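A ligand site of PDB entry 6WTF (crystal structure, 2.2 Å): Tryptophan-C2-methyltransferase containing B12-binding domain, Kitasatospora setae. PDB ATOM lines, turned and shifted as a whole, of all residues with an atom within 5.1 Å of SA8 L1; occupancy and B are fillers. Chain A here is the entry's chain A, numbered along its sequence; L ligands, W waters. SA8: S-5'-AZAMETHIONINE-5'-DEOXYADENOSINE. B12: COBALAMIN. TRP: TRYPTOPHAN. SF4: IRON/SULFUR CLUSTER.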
ATOM      1  N   VAL A  74      24.107  25.745  32.834  1.00  0.00           N
ATOM      2  CA  VAL A  74      23.738  26.097  31.469  1.00  0.00           C
ATOM      3  C   VAL A  74      23.009  27.440  31.472  1.00  0.00           C
ATOM      4  O   VAL A  74      21.932  27.588  30.881  1.00  0.00           O
ATOM      5  CB  VAL A  74      22.917  24.969  30.811  1.00  0.00           C
ATOM      6  CG1 VAL A  74      22.755  25.216  29.298  1.00  0.00           C
ATOM      7  CG2 VAL A  74      23.601  23.643  31.042  1.00  0.00           C
ATOM      8  N   HIS A 233      20.874  24.596  19.395  1.00  0.00           N
ATOM      9  CA  HIS A 233      21.287  24.943  20.744  1.00  0.00           C
ATOM     10  C   HIS A 233      21.302  23.743  21.689  1.00  0.00           C
ATOM     11  O   HIS A 233      21.869  23.855  22.787  1.00  0.00           O
ATOM     12  CB  HIS A 233      20.326  25.995  21.316  1.00  0.00           C
ATOM     13  CG  HIS A 233      18.964  25.453  21.641  1.00  0.00           C
ATOM     14  ND1 HIS A 233      17.978  25.304  20.685  1.00  0.00           N
ATOM     15  CD2 HIS A 233      18.435  24.996  22.796  1.00  0.00           C
ATOM     16  CE1 HIS A 233      16.902  24.800  21.249  1.00  0.00           C
ATOM     17  NE2 HIS A 233      17.150  24.600  22.527  1.00  0.00           N
ATOM     18  N   CYS A 234      20.715  22.622  21.310  1.00  0.00           N
ATOM     19  CA  CYS A 234      20.262  21.608  22.267  1.00  0.00           C
ATOM     20  C   CYS A 234      21.176  20.393  22.247  1.00  0.00           C
ATOM     21  O   CYS A 234      21.443  19.823  21.177  1.00  0.00           O
ATOM     22  CB  CYS A 234      18.827  21.192  21.953  1.00  0.00           C
ATOM     23  SG  CYS A 234      18.030  20.294  23.288  1.00  0.00           S
ATOM     24  N   GLU A 236      20.359  17.488  23.592  1.00  0.00           N
ATOM     25  CA  GLU A 236      19.602  16.263  23.831  1.00  0.00           C
ATOM     26  C   GLU A 236      19.596  15.286  22.669  1.00  0.00           C
ATOM     27  O   GLU A 236      19.699  14.070  22.900  1.00  0.00           O
ATOM     28  CB  GLU A 236      18.151  16.580  24.249  1.00  0.00           C
ATOM     29  CG  GLU A 236      18.064  17.424  25.504  1.00  0.00           C
ATOM     30  CD  GLU A 236      16.663  17.480  26.084  1.00  0.00           C
ATOM     31  OE1 GLU A 236      15.890  16.516  25.898  1.00  0.00           O
ATOM     32  OE2 GLU A 236      16.324  18.496  26.714  1.00  0.00           O
ATOM     33  N   ASP A 271      10.457  13.593  29.161  1.00  0.00           N
ATOM     34  CA  ASP A 271      10.749  13.479  27.746  1.00  0.00           C
ATOM     35  C   ASP A 271      11.497  14.713  27.268  1.00  0.00           C
ATOM     36  O   ASP A 271      11.452  15.786  27.883  1.00  0.00           O
ATOM     37  CB  ASP A 271       9.458  13.347  26.936  1.00  0.00           C
ATOM     38  CG  ASP A 271       8.609  12.175  27.377  1.00  0.00           C
ATOM     39  OD1 ASP A 271       9.139  11.260  28.041  1.00  0.00           O
ATOM     40  OD2 ASP A 271       7.403  12.170  27.058  1.00  0.00           O
ATOM     41  N   SER A 272      12.220  14.557  26.154  1.00  0.00           N
ATOM     42  CA  SER A 272      12.777  15.725  25.485  1.00  0.00           C
ATOM     43  C   SER A 272      11.680  16.726  25.166  1.00  0.00           C
ATOM     44  O   SER A 272      11.790  17.909  25.500  1.00  0.00           O
ATOM     45  CB  SER A 272      13.519  15.302  24.217  1.00  0.00           C
ATOM     46  OG  SER A 272      14.734  14.647  24.546  1.00  0.00           O
ATOM     47  N   GLU A 273      10.606  16.264  24.535  1.00  0.00           N
ATOM     48  CA  GLU A 273       9.407  17.061  24.292  1.00  0.00           C
ATOM     49  C   GLU A 273       8.214  16.127  24.360  1.00  0.00           C
ATOM     50  O   GLU A 273       8.164  15.136  23.629  1.00  0.00           O
ATOM     51  CB  GLU A 273       9.455  17.754  22.924  1.00  0.00           C
ATOM     52  CG  GLU A 273      10.678  18.600  22.659  1.00  0.00           C
ATOM     53  CD  GLU A 273      10.708  19.888  23.457  1.00  0.00           C
ATOM     54  OE1 GLU A 273       9.684  20.252  24.066  1.00  0.00           O
ATOM     55  OE2 GLU A 273      11.760  20.541  23.463  1.00  0.00           O
ATOM     56  N   TYR A 308       6.762  19.363  29.050  1.00  0.00           N
ATOM     57  CA  TYR A 308       7.484  20.167  28.066  1.00  0.00           C
ATOM     58  C   TYR A 308       6.836  19.976  26.701  1.00  0.00           C
ATOM     59  O   TYR A 308       6.443  18.868  26.343  1.00  0.00           O
ATOM     60  CB  TYR A 308       8.957  19.768  27.983  1.00  0.00           C
ATOM     61  CG  TYR A 308       9.887  20.438  28.967  1.00  0.00           C
ATOM     62  CD1 TYR A 308       9.764  21.780  29.276  1.00  0.00           C
ATOM     63  CD2 TYR A 308      10.899  19.712  29.590  1.00  0.00           C
ATOM     64  CE1 TYR A 308      10.622  22.400  30.179  1.00  0.00           C
ATOM     65  CE2 TYR A 308      11.759  20.311  30.486  1.00  0.00           C
ATOM     66  CZ  TYR A 308      11.619  21.641  30.787  1.00  0.00           C
ATOM     67  OH  TYR A 308      12.484  22.226  31.681  1.00  0.00           O
ATOM     68  N   GLN A 310       6.930  21.557  22.387  1.00  0.00           N
ATOM     69  CA  GLN A 310       7.244  22.465  21.303  1.00  0.00           C
ATOM     70  C   GLN A 310       5.940  23.059  20.778  1.00  0.00           C
ATOM     71  O   GLN A 310       4.865  22.497  21.005  1.00  0.00           O
ATOM     72  CB  GLN A 310       7.996  21.739  20.193  1.00  0.00           C
ATOM     73  CG  GLN A 310       9.449  21.492  20.518  1.00  0.00           C
ATOM     74  CD  GLN A 310      10.223  22.775  20.653  1.00  0.00           C
ATOM     75  OE1 GLN A 310      10.440  23.498  19.676  1.00  0.00           O
ATOM     76  NE2 GLN A 310      10.650  23.081  21.871  1.00  0.00           N
ATOM     77  N   ASN A 331       5.070  24.011  29.543  1.00  0.00           N
ATOM     78  CA  ASN A 331       6.204  24.864  29.193  1.00  0.00           C
ATOM     79  C   ASN A 331       6.492  24.639  27.716  1.00  0.00           C
ATOM     80  O   ASN A 331       6.784  23.517  27.309  1.00  0.00           O
ATOM     81  CB  ASN A 331       7.423  24.553  30.058  1.00  0.00           C
ATOM     82  CG  ASN A 331       8.631  25.401  29.725  1.00  0.00           C
ATOM     83  OD1 ASN A 331       9.106  25.398  28.591  1.00  0.00           O
ATOM     84  ND2 ASN A 331       9.134  26.127  30.707  1.00  0.00           N
ATOM     85  N   GLY A 333       8.795  25.735  24.457  1.00  0.00           N
ATOM     86  CA  GLY A 333      10.019  26.365  24.019  1.00  0.00           C
ATOM     87  C   GLY A 333       9.867  27.061  22.677  1.00  0.00           C
ATOM     88  O   GLY A 333      10.471  26.653  21.684  1.00  0.00           O
ATOM     89  N   ASP A 335      10.976  30.000  21.984  1.00  0.00           N
ATOM     90  CA  ASP A 335      12.368  30.423  21.811  1.00  0.00           C
ATOM     91  C   ASP A 335      12.523  31.731  21.034  1.00  0.00           C
ATOM     92  O   ASP A 335      13.362  32.562  21.397  1.00  0.00           O
ATOM     93  CB  ASP A 335      13.189  29.300  21.189  1.00  0.00           C
ATOM     94  CG  ASP A 335      13.342  28.110  22.139  1.00  0.00           C
ATOM     95  OD1 ASP A 335      13.264  28.336  23.365  1.00  0.00           O
ATOM     96  OD2 ASP A 335      13.543  26.972  21.671  1.00  0.00           O
ATOM     97  N   GLU A 377       9.047  30.094  26.650  1.00  0.00           N
ATOM     98  CA  GLU A 377      10.489  30.310  26.699  1.00  0.00           C
ATOM     99  C   GLU A 377      10.944  31.200  25.547  1.00  0.00           C
ATOM    100  O   GLU A 377      10.467  31.063  24.419  1.00  0.00           O
ATOM    101  CB  GLU A 377      11.252  28.980  26.633  1.00  0.00           C
ATOM    102  CG  GLU A 377      10.894  27.954  27.708  1.00  0.00           C
ATOM    103  CD  GLU A 377      11.723  28.110  28.976  1.00  0.00           C
ATOM    104  OE1 GLU A 377      12.388  29.145  29.137  1.00  0.00           O
ATOM    105  OE2 GLU A 377      11.687  27.182  29.817  1.00  0.00           O
ATOM    106  N   ALA A 378      11.870  32.107  25.839  1.00  0.00           N
ATOM    107  CA  ALA A 378      12.548  32.906  24.831  1.00  0.00           C
ATOM    108  C   ALA A 378      14.044  32.857  25.095  1.00  0.00           C
ATOM    109  O   ALA A 378      14.483  33.078  26.232  1.00  0.00           O
ATOM    110  CB  ALA A 378      12.059  34.358  24.835  1.00  0.00           C
ATOM    111  N   LEU A 379      14.836  32.555  24.056  1.00  0.00           N
ATOM    112  CA  LEU A 379      16.284  32.469  24.165  1.00  0.00           C
ATOM    113  C   LEU A 379      16.906  33.519  23.253  1.00  0.00           C
ATOM    114  O   LEU A 379      16.782  33.429  22.024  1.00  0.00           O
ATOM    115  CB  LEU A 379      16.806  31.072  23.829  1.00  0.00           C
ATOM    116  CG  LEU A 379      18.314  30.885  23.971  1.00  0.00           C
ATOM    117  CD1 LEU A 379      18.787  31.295  25.358  1.00  0.00           C
ATOM    118  CD2 LEU A 379      18.733  29.442  23.680  1.00  0.00           C
ATOM    119  N   SER A 408      15.694  34.368  28.507  1.00  0.00           N
ATOM    120  CA  SER A 408      17.103  34.056  28.732  1.00  0.00           C
ATOM    121  C   SER A 408      17.949  34.703  27.638  1.00  0.00           C
ATOM    122  O   SER A 408      17.483  34.944  26.525  1.00  0.00           O
ATOM    123  CB  SER A 408      17.313  32.535  28.753  1.00  0.00           C
ATOM    124  OG  SER A 408      16.412  31.927  29.663  1.00  0.00           O
ATOM    125  N   GLY A 410      21.848  34.601  25.910  1.00  0.00           N
ATOM    126  CA  GLY A 410      23.155  33.984  25.764  1.00  0.00           C
ATOM    127  C   GLY A 410      23.056  32.470  25.676  1.00  0.00           C
ATOM    128  O   GLY A 410      22.210  31.832  26.316  1.00  0.00           O
ATOM    129  N   LEU A 411      23.977  31.881  24.907  1.00  0.00           N
ATOM    130  CA  LEU A 411      23.952  30.460  24.598  1.00  0.00           C
ATOM    131  C   LEU A 411      25.211  29.793  25.119  1.00  0.00           C
ATOM    132  O   LEU A 411      26.322  30.259  24.835  1.00  0.00           O
ATOM    133  CB  LEU A 411      23.833  30.235  23.094  1.00  0.00           C
ATOM    134  CG  LEU A 411      23.933  28.776  22.673  1.00  0.00           C
ATOM    135  CD1 LEU A 411      22.650  28.055  23.032  1.00  0.00           C
ATOM    136  CD2 LEU A 411      24.248  28.651  21.184  1.00  0.00           C
ATOM    137  N   ARG A 412      25.040  28.704  25.871  1.00  0.00           N
ATOM    138  CA  ARG A 412      26.168  27.877  26.270  1.00  0.00           C
ATOM    139  C   ARG A 412      26.496  26.888  25.156  1.00  0.00           C
ATOM    140  O   ARG A 412      25.607  26.206  24.647  1.00  0.00           O
ATOM    141  CB  ARG A 412      25.851  27.144  27.567  1.00  0.00           C
ATOM    142  CG  ARG A 412      26.072  27.979  28.810  1.00  0.00           C
ATOM    143  CD  ARG A 412      27.498  27.802  29.316  1.00  0.00           C
ATOM    144  NE  ARG A 412      27.745  26.435  29.738  1.00  0.00           N
ATOM    145  CZ  ARG A 412      28.631  25.624  29.177  1.00  0.00           C
ATOM    146  NH1 ARG A 412      29.376  26.045  28.152  1.00  0.00           N
ATOM    147  NH2 ARG A 412      28.783  24.389  29.632  1.00  0.00           N
ATOM    148  N   PHE A 414      28.309  23.553  23.421  1.00  0.00           N
ATOM    149  CA  PHE A 414      28.611  22.168  23.753  1.00  0.00           C
ATOM    150  C   PHE A 414      29.097  21.461  22.495  1.00  0.00           C
ATOM    151  O   PHE A 414      28.699  21.824  21.388  1.00  0.00           O
ATOM    152  CB  PHE A 414      27.367  21.447  24.306  1.00  0.00           C
ATOM    153  CG  PHE A 414      27.054  21.824  25.733  1.00  0.00           C
ATOM    154  CD1 PHE A 414      26.169  22.864  26.004  1.00  0.00           C
ATOM    155  CD2 PHE A 414      27.630  21.148  26.786  1.00  0.00           C
ATOM    156  CE1 PHE A 414      25.876  23.214  27.317  1.00  0.00           C
ATOM    157  CE2 PHE A 414      27.343  21.486  28.095  1.00  0.00           C
ATOM    158  CZ  PHE A 414      26.469  22.524  28.358  1.00  0.00           C
ATOM    159  N   ASN A 527      15.604  33.066  34.805  1.00  0.00           N
ATOM    160  CA  ASN A 527      15.075  31.764  34.432  1.00  0.00           C
ATOM    161  C   ASN A 527      16.123  30.713  34.776  1.00  0.00           C
ATOM    162  O   ASN A 527      16.780  30.177  33.882  1.00  0.00           O
ATOM    163  CB  ASN A 527      14.729  31.742  32.930  1.00  0.00           C
ATOM    164  CG  ASN A 527      13.973  30.490  32.506  1.00  0.00           C
ATOM    165  OD1 ASN A 527      13.840  29.527  33.257  1.00  0.00           O
ATOM    166  ND2 ASN A 527      13.489  30.503  31.265  1.00  0.00           N
HETATM  167  N   SA8 L   1      13.767  19.383  26.605  1.00  0.00           N
HETATM  168  CA  SA8 L   1      14.125  20.809  26.565  1.00  0.00           C
HETATM  169  C   SA8 L   1      15.085  21.147  27.700  1.00  0.00           C
HETATM  170  O   SA8 L   1      15.938  22.066  27.368  1.00  0.00           O
HETATM  171  OXT SA8 L   1      15.044  20.605  28.786  1.00  0.00           O
HETATM  172  CB  SA8 L   1      12.866  21.725  26.632  1.00  0.00           C
HETATM  173  CG  SA8 L   1      13.085  23.069  25.950  1.00  0.00           C
HETATM  174  ND  SA8 L   1      13.901  23.999  26.734  1.00  0.00           N
HETATM  175  CE  SA8 L   1      13.258  24.287  28.023  1.00  0.00           C
HETATM  176  C5' SA8 L   1      14.255  25.192  25.968  1.00  0.00           C
HETATM  177  C4' SA8 L   1      15.034  26.211  26.773  1.00  0.00           C
HETATM  178  O4' SA8 L   1      16.209  25.588  27.354  1.00  0.00           O
HETATM  179  C3' SA8 L   1      15.618  27.333  25.920  1.00  0.00           C
HETATM  180  O3' SA8 L   1      14.643  28.345  25.669  1.00  0.00           O
HETATM  181  C2' SA8 L   1      16.758  27.841  26.802  1.00  0.00           C
HETATM  182  O2' SA8 L   1      16.284  28.776  27.762  1.00  0.00           O
HETATM  183  C1' SA8 L   1      17.229  26.549  27.492  1.00  0.00           C
HETATM  184  N9  SA8 L   1      18.469  25.996  26.937  1.00  0.00           N
HETATM  185  C8  SA8 L   1      18.637  24.767  26.363  1.00  0.00           C
HETATM  186  N7  SA8 L   1      19.857  24.545  25.930  1.00  0.00           N
HETATM  187  C5  SA8 L   1      20.544  25.704  26.260  1.00  0.00           C
HETATM  188  C6  SA8 L   1      21.883  26.108  26.077  1.00  0.00           C
HETATM  189  N6  SA8 L   1      22.808  25.367  25.452  1.00  0.00           N
HETATM  190  N1  SA8 L   1      22.239  27.321  26.550  1.00  0.00           N
HETATM  191  C2  SA8 L   1      21.318  28.087  27.140  1.00  0.00           C
HETATM  192  N3  SA8 L   1      20.019  27.820  27.349  1.00  0.00           N
HETATM  193  C4  SA8 L   1      19.698  26.611  26.887  1.00  0.00           C
HETATM  194 CO   B12 L   2      16.697  20.079  33.303  1.00  0.00          CO
HETATM  195  N21 B12 L   2      18.292  19.798  32.334  1.00  0.00           N
HETATM  196  N22 B12 L   2      17.648  21.250  34.489  1.00  0.00           N
HETATM  197  N23 B12 L   2      15.107  19.966  34.375  1.00  0.00           N
HETATM  198  N24 B12 L   2      16.013  18.746  32.139  1.00  0.00           N
HETATM  199  C1  B12 L   2      18.346  18.744  31.335  1.00  0.00           C
HETATM  200  C20 B12 L   2      18.976  17.523  31.982  1.00  0.00           C
HETATM  201  C2  B12 L   2      19.174  19.410  30.166  1.00  0.00           C
HETATM  202  C25 B12 L   2      19.904  18.415  29.250  1.00  0.00           C
HETATM  203  C26 B12 L   2      18.316  20.342  29.284  1.00  0.00           C
HETATM  204  C27 B12 L   2      19.001  20.774  27.985  1.00  0.00           C
HETATM  205  O28 B12 L   2      20.023  21.465  28.040  1.00  0.00           O
HETATM  206  N29 B12 L   2      18.471  20.382  26.842  1.00  0.00           N
HETATM  207  C3  B12 L   2      20.138  20.350  30.969  1.00  0.00           C
HETATM  208  C30 B12 L   2      21.494  19.720  31.343  1.00  0.00           C
HETATM  209  C31 B12 L   2      22.657  20.210  30.469  1.00  0.00           C
HETATM  210  C32 B12 L   2      24.028  19.742  30.914  1.00  0.00           C
HETATM  211  O34 B12 L   2      24.188  19.204  32.008  1.00  0.00           O
HETATM  212  N33 B12 L   2      25.019  19.943  30.059  1.00  0.00           N
HETATM  213  C4  B12 L   2      19.257  20.655  32.161  1.00  0.00           C
HETATM  214  C5  B12 L   2      19.487  21.818  33.041  1.00  0.00           C
HETATM  215  C35 B12 L   2      20.569  22.720  32.532  1.00  0.00           C
HETATM  216  C6  B12 L   2      18.784  22.002  34.202  1.00  0.00           C
HETATM  217  C7  B12 L   2      18.983  23.045  35.295  1.00  0.00           C
HETATM  218  C36 B12 L   2      20.438  23.137  35.783  1.00  0.00           C
HETATM  219  C37 B12 L   2      18.427  24.400  34.779  1.00  0.00           C
HETATM  220  C38 B12 L   2      18.622  25.539  35.795  1.00  0.00           C
HETATM  221  O39 B12 L   2      17.895  25.619  36.794  1.00  0.00           O
HETATM  222  N40 B12 L   2      19.589  26.409  35.539  1.00  0.00           N
HETATM  223  C8  B12 L   2      18.078  22.495  36.441  1.00  0.00           C
HETATM  224  C41 B12 L   2      18.783  21.538  37.417  1.00  0.00           C
HETATM  225  C42 B12 L   2      17.873  21.018  38.530  1.00  0.00           C
HETATM  226  C43 B12 L   2      18.524  20.010  39.463  1.00  0.00           C
HETATM  227  O44 B12 L   2      19.407  19.245  39.059  1.00  0.00           O
HETATM  228  N45 B12 L   2      18.080  20.006  40.711  1.00  0.00           N
HETATM  229  C9  B12 L   2      17.088  21.706  35.619  1.00  0.00           C
HETATM  230  C10 B12 L   2      15.771  21.599  36.010  1.00  0.00           C
HETATM  231  C11 B12 L   2      14.830  20.828  35.359  1.00  0.00           C
HETATM  232  C12 B12 L   2      13.368  20.767  35.762  1.00  0.00           C
HETATM  233  C46 B12 L   2      13.179  20.883  37.281  1.00  0.00           C
HETATM  234  C47 B12 L   2      12.615  21.910  35.068  1.00  0.00           C
HETATM  235  C13 B12 L   2      12.965  19.337  35.289  1.00  0.00           C
HETATM  236  C48 B12 L   2      13.052  18.241  36.354  1.00  0.00           C
HETATM  237  C49 B12 L   2      11.698  17.634  36.735  1.00  0.00           C
HETATM  238  C50 B12 L   2      11.789  16.453  37.673  1.00  0.00           C
HETATM  239  O51 B12 L   2      12.569  15.527  37.459  1.00  0.00           O
HETATM  240  N52 B12 L   2      10.981  16.485  38.721  1.00  0.00           N
HETATM  241  C14 B12 L   2      14.025  19.101  34.189  1.00  0.00           C
HETATM  242  C15 B12 L   2      13.867  18.184  33.195  1.00  0.00           C
HETATM  243  C53 B12 L   2      12.594  17.383  33.125  1.00  0.00           C
HETATM  244  C16 B12 L   2      14.988  17.930  32.203  1.00  0.00           C
HETATM  245  C17 B12 L   2      15.017  16.834  31.139  1.00  0.00           C
HETATM  246  C54 B12 L   2      14.068  17.169  29.970  1.00  0.00           C
HETATM  247  C55 B12 L   2      14.730  15.380  31.613  1.00  0.00           C
HETATM  248  C56 B12 L   2      15.622  14.922  32.768  1.00  0.00           C
HETATM  249  C57 B12 L   2      15.223  13.512  33.120  1.00  0.00           C
HETATM  250  O58 B12 L   2      14.774  13.239  34.240  1.00  0.00           O
HETATM  251  N59 B12 L   2      15.365  12.603  32.162  1.00  0.00           N
HETATM  252  C18 B12 L   2      16.508  16.888  30.751  1.00  0.00           C
HETATM  253  C60 B12 L   2      16.890  16.403  29.338  1.00  0.00           C
HETATM  254  C61 B12 L   2      16.607  14.935  29.067  1.00  0.00           C
HETATM  255  O63 B12 L   2      16.981  14.070  29.872  1.00  0.00           O
HETATM  256  N62 B12 L   2      15.939  14.657  27.961  1.00  0.00           N
HETATM  257  C19 B12 L   2      16.862  18.360  30.998  1.00  0.00           C
HETATM  258  C1P B12 L   2      15.016  11.197  32.331  1.00  0.00           C
HETATM  259  C2P B12 L   2      16.150  10.426  33.090  1.00  0.00           C
HETATM  260  C3P B12 L   2      15.675   9.052  33.490  1.00  0.00           C
HETATM  261  O3  B12 L   2      17.212  10.228  32.189  1.00  0.00           O
HETATM  262  O4  B12 L   2      19.434  11.219  31.313  1.00  0.00           O
HETATM  263  O5  B12 L   2      18.890  11.296  33.763  1.00  0.00           O
HETATM  264  P   B12 L   2      18.748  10.543  32.449  1.00  0.00           P
HETATM  265  O2  B12 L   2      19.289   9.080  32.803  1.00  0.00           O
HETATM  266  C3R B12 L   2      19.569   8.047  31.880  1.00  0.00           C
HETATM  267  C2R B12 L   2      20.909   8.189  31.158  1.00  0.00           C
HETATM  268  O7R B12 L   2      21.436   9.499  31.337  1.00  0.00           O
HETATM  269  C1R B12 L   2      21.756   7.104  31.842  1.00  0.00           C
HETATM  270  O6R B12 L   2      20.859   6.074  32.201  1.00  0.00           O
HETATM  271  C4R B12 L   2      19.629   6.692  32.607  1.00  0.00           C
HETATM  272  C5R B12 L   2      18.470   5.762  32.325  1.00  0.00           C
HETATM  273  O8R B12 L   2      18.207   5.653  30.934  1.00  0.00           O
HETATM  274  N1B B12 L   2      22.497   7.527  33.028  1.00  0.00           N
HETATM  275  C8B B12 L   2      23.515   6.784  33.604  1.00  0.00           C
HETATM  276  C2B B12 L   2      22.178   8.498  33.942  1.00  0.00           C
HETATM  277  N3B B12 L   2      22.894   8.454  35.034  1.00  0.00           N
HETATM  278  C9B B12 L   2      23.748   7.365  34.847  1.00  0.00           C
HETATM  279  C4B B12 L   2      24.725   6.840  35.684  1.00  0.00           C
HETATM  280  C5B B12 L   2      25.471   5.737  35.269  1.00  0.00           C
HETATM  281  C5M B12 L   2      26.506   5.166  36.203  1.00  0.00           C
HETATM  282  C6B B12 L   2      25.230   5.159  34.002  1.00  0.00           C
HETATM  283  C6M B12 L   2      26.041   3.972  33.530  1.00  0.00           C
HETATM  284  C7B B12 L   2      24.242   5.686  33.173  1.00  0.00           C
HETATM  285  N   TRP L   3      13.349  27.175  31.839  1.00  0.00           N
HETATM  286  CA  TRP L   3      13.324  25.761  32.208  1.00  0.00           C
HETATM  287  C   TRP L   3      11.954  25.382  32.752  1.00  0.00           C
HETATM  288  O   TRP L   3      11.637  24.196  32.876  1.00  0.00           O
HETATM  289  CB  TRP L   3      14.417  25.448  33.247  1.00  0.00           C
HETATM  290  CG  TRP L   3      15.777  25.977  32.873  1.00  0.00           C
HETATM  291  CD1 TRP L   3      16.380  27.084  33.371  1.00  0.00           C
HETATM  292  CD2 TRP L   3      16.684  25.415  31.903  1.00  0.00           C
HETATM  293  NE1 TRP L   3      17.612  27.257  32.785  1.00  0.00           N
HETATM  294  CE2 TRP L   3      17.822  26.245  31.884  1.00  0.00           C
HETATM  295  CE3 TRP L   3      16.641  24.305  31.067  1.00  0.00           C
HETATM  296  CZ2 TRP L   3      18.908  25.994  31.047  1.00  0.00           C
HETATM  297  CZ3 TRP L   3      17.726  24.051  30.239  1.00  0.00           C
HETATM  298  CH2 TRP L   3      18.845  24.890  30.240  1.00  0.00           C
HETATM  299  OXT TRP L   3      11.153  26.256  33.073  1.00  0.00           O
HETATM  300 FE1  SF4 L   4      14.677  20.902  19.861  1.00  0.00          FE
HETATM  301 FE2  SF4 L   4      14.482  18.306  20.721  1.00  0.00          FE
HETATM  302 FE3  SF4 L   4      13.380  20.328  22.197  1.00  0.00          FE
HETATM  303 FE4  SF4 L   4      16.088  20.068  22.062  1.00  0.00          FE
HETATM  304  S1  SF4 L   4      14.630  18.589  22.972  1.00  0.00           S
HETATM  305  S2  SF4 L   4      14.879  22.001  21.856  1.00  0.00           S
HETATM  306  S3  SF4 L   4      16.352  19.342  19.924  1.00  0.00           S
HETATM  307  S4  SF4 L   4      12.778  19.677  20.094  1.00  0.00           S
HETATM  308  O   HOH W   1      15.421  21.449  31.325  1.00  0.00           O
HETATM  309  O   HOH W   2      15.448  28.117  30.337  1.00  0.00           O
HETATM  310  O   HOH W   3       9.770  22.754  25.848  1.00  0.00           O
HETATM  311  O   HOH W   4      14.454  30.913  28.157  1.00  0.00           O
HETATM  312  O   HOH W   5      19.549  29.764  29.427  1.00  0.00           O
HETATM  313  O   HOH W   6      21.110  21.964  25.549  1.00  0.00           O
HETATM  314  O   HOH W   7      16.846  22.627  25.092  1.00  0.00           O
HETATM  315  O   HOH W   8      12.835  24.595  22.848  1.00  0.00           O
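An oxygen (O3') of SA8 L1 is in hydrogen-bond range of the side-chain carboxylate (OD1) of Asp 335 (2.7 Å). The backbone carbonyl oxygen of Ser 272 is in hydrogen-bond range of a nitrogen (N) of SA8 L1, at 2.7 Å. The side-chain carboxylate of Glu 236 is in salt-bridge range of a nitrogen (N) of SA8 L1 (2.7 Å). N of Arg 412 lies within hydrogen-bond range of N1 of SA8 L1. A nitrogen (N6) of SA8 L1 lies within hydrogen-bond range of the backbone carbonyl oxygen of Arg 412, at 3.0 Å. The backbone carbonyl oxygen of His 233 sits at hydrogen-bond distance from a nitrogen (N6) of SA8 L1 (3.2 Å). The side-chain carboxylate of Glu 273 sits close to a nitrogen (N) of SA8 L1, at 3.9 Å. OE1 of Glu 236 is in hydrogen-bond range of N62 of B12 L2 (2.8 Å). SG of Cys 234 lies close to N29 of B12 L2 (3.6 Å). The side-chain carboxylate of Glu 377 lies within salt-bridge range of a nitrogen (N) of TRP L3, at 2.6 Å. The side-chain hydroxyl of Tyr 308 is in hydrogen-bond range of an oxygen (O) of TRP L3 (2.5 Å). OXT of TRP L3 sits at hydrogen-bond distance from ND2 of Asn 331 (3.1 Å). The backbone carbonyl oxygen of Asn 527 sits close to a nitrogen (NE1) of TRP L3 (3.2 Å). N of TRP L3 lies within hydrogen-bond range of OD1 of Asn 527, at 2.8 Å. A ring nitrogen (NE2) of His 233 lies close to a sulfur (S2) of SF4 L4. The side-chain carboxylate (OE2) of Glu 273 binds an iron atom (FE3) of SF4 L4, at 2.1 Å. An iron atom (FE4) of SF4 L4 is bound by the side-chain sulfur (SG) of Cys 234 (2.3 Å).
A nitrogen (N29) of B12 L2 lies within hydrogen-bond range of an oxygen (O) of SA8 L1 (3.1 Å).
The backbone carbonyl oxygen of Glu 377 is in hydrogen-bond range of the backbone NH of Asp 335, 2.7 Å away. The backbone NH of Leu 379 lies within hydrogen-bond range of the backbone carbonyl oxygen of Asp 335 (3.0 Å). OG of Ser 272 is in hydrogen-bond range of OE1 of Glu 236 (2.6 Å). N of Glu 236 sits close to SG of Cys 234 (3.7 Å). OE1 of Glu 273 is in hydrogen-bond range of N of Gln 310, at 3.5 Å. The side-chain amide nitrogen of Asn 331 lies within hydrogen-bond range of the side-chain carboxylate of Glu 377 (2.9 Å). OE1 of Glu 377 sits at hydrogen-bond distance from ND2 of Asn 527, at 2.8 Å. N of Ser 408 lies within hydrogen-bond range of O of Ala 378 (2.9 Å).
Val 74 touches SA8 L1 (CG1 to C6, 3.5 Å). CE2 of Tyr 308 touches OXT of SA8 L1, 3.7 Å away. Glu 377 touches SA8 L1. Leu 379 touches SA8 L1 (CB to O3', 3.9 Å). Ser 408 touches SA8 L1. O of Gly 410 touches C2 of SA8 L1, at 3.9 Å. Leu 411 touches SA8 L1 (CD1 to N1, 3.6 Å). Hydrophobic or aromatic side chains within 4 Å of SA8 L1: Val 74, His 233, Tyr 308, Leu 379 and Leu 411. Along chain A the residues within 4 Å of SA8 L1 span positions 74 to 412. The nearest printed residue that does not touch SA8 L1 is Phe 414 (4.2 Å).
Water W7 lies within hydrogen-bond range of an oxygen (O) of SA8 L1 (2.5 Å), a ring nitrogen (NE2) of His 233 (3.3 Å) and a nitrogen (N29) of B12 L2 (3.3 Å). Water W1 lies within hydrogen-bond range of OXT of SA8 L1 (2.7 Å) and OH of Tyr 308 (3.1 Å). Water W2 lies within hydrogen-bond range of a nitrogen (N) of TRP L3 (2.7 Å), an oxygen (O2') of SA8 L1 (2.8 Å), the side-chain amide nitrogen of Asn 527 (3.2 Å) and the side-chain carboxylate of Glu 377 (3.4 Å). Water W4 lies within hydrogen-bond range of OG of Ser 408, O2' of SA8 L1, OE1 of Glu 377, O of Ala 378 and ND2 of Asn 527. Water W3 lies within hydrogen-bond range of OE1 of Glu 273 (3.1 Å), O of Asn 331 (3.4 Å) and N of Gly 333 (3.4 Å).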
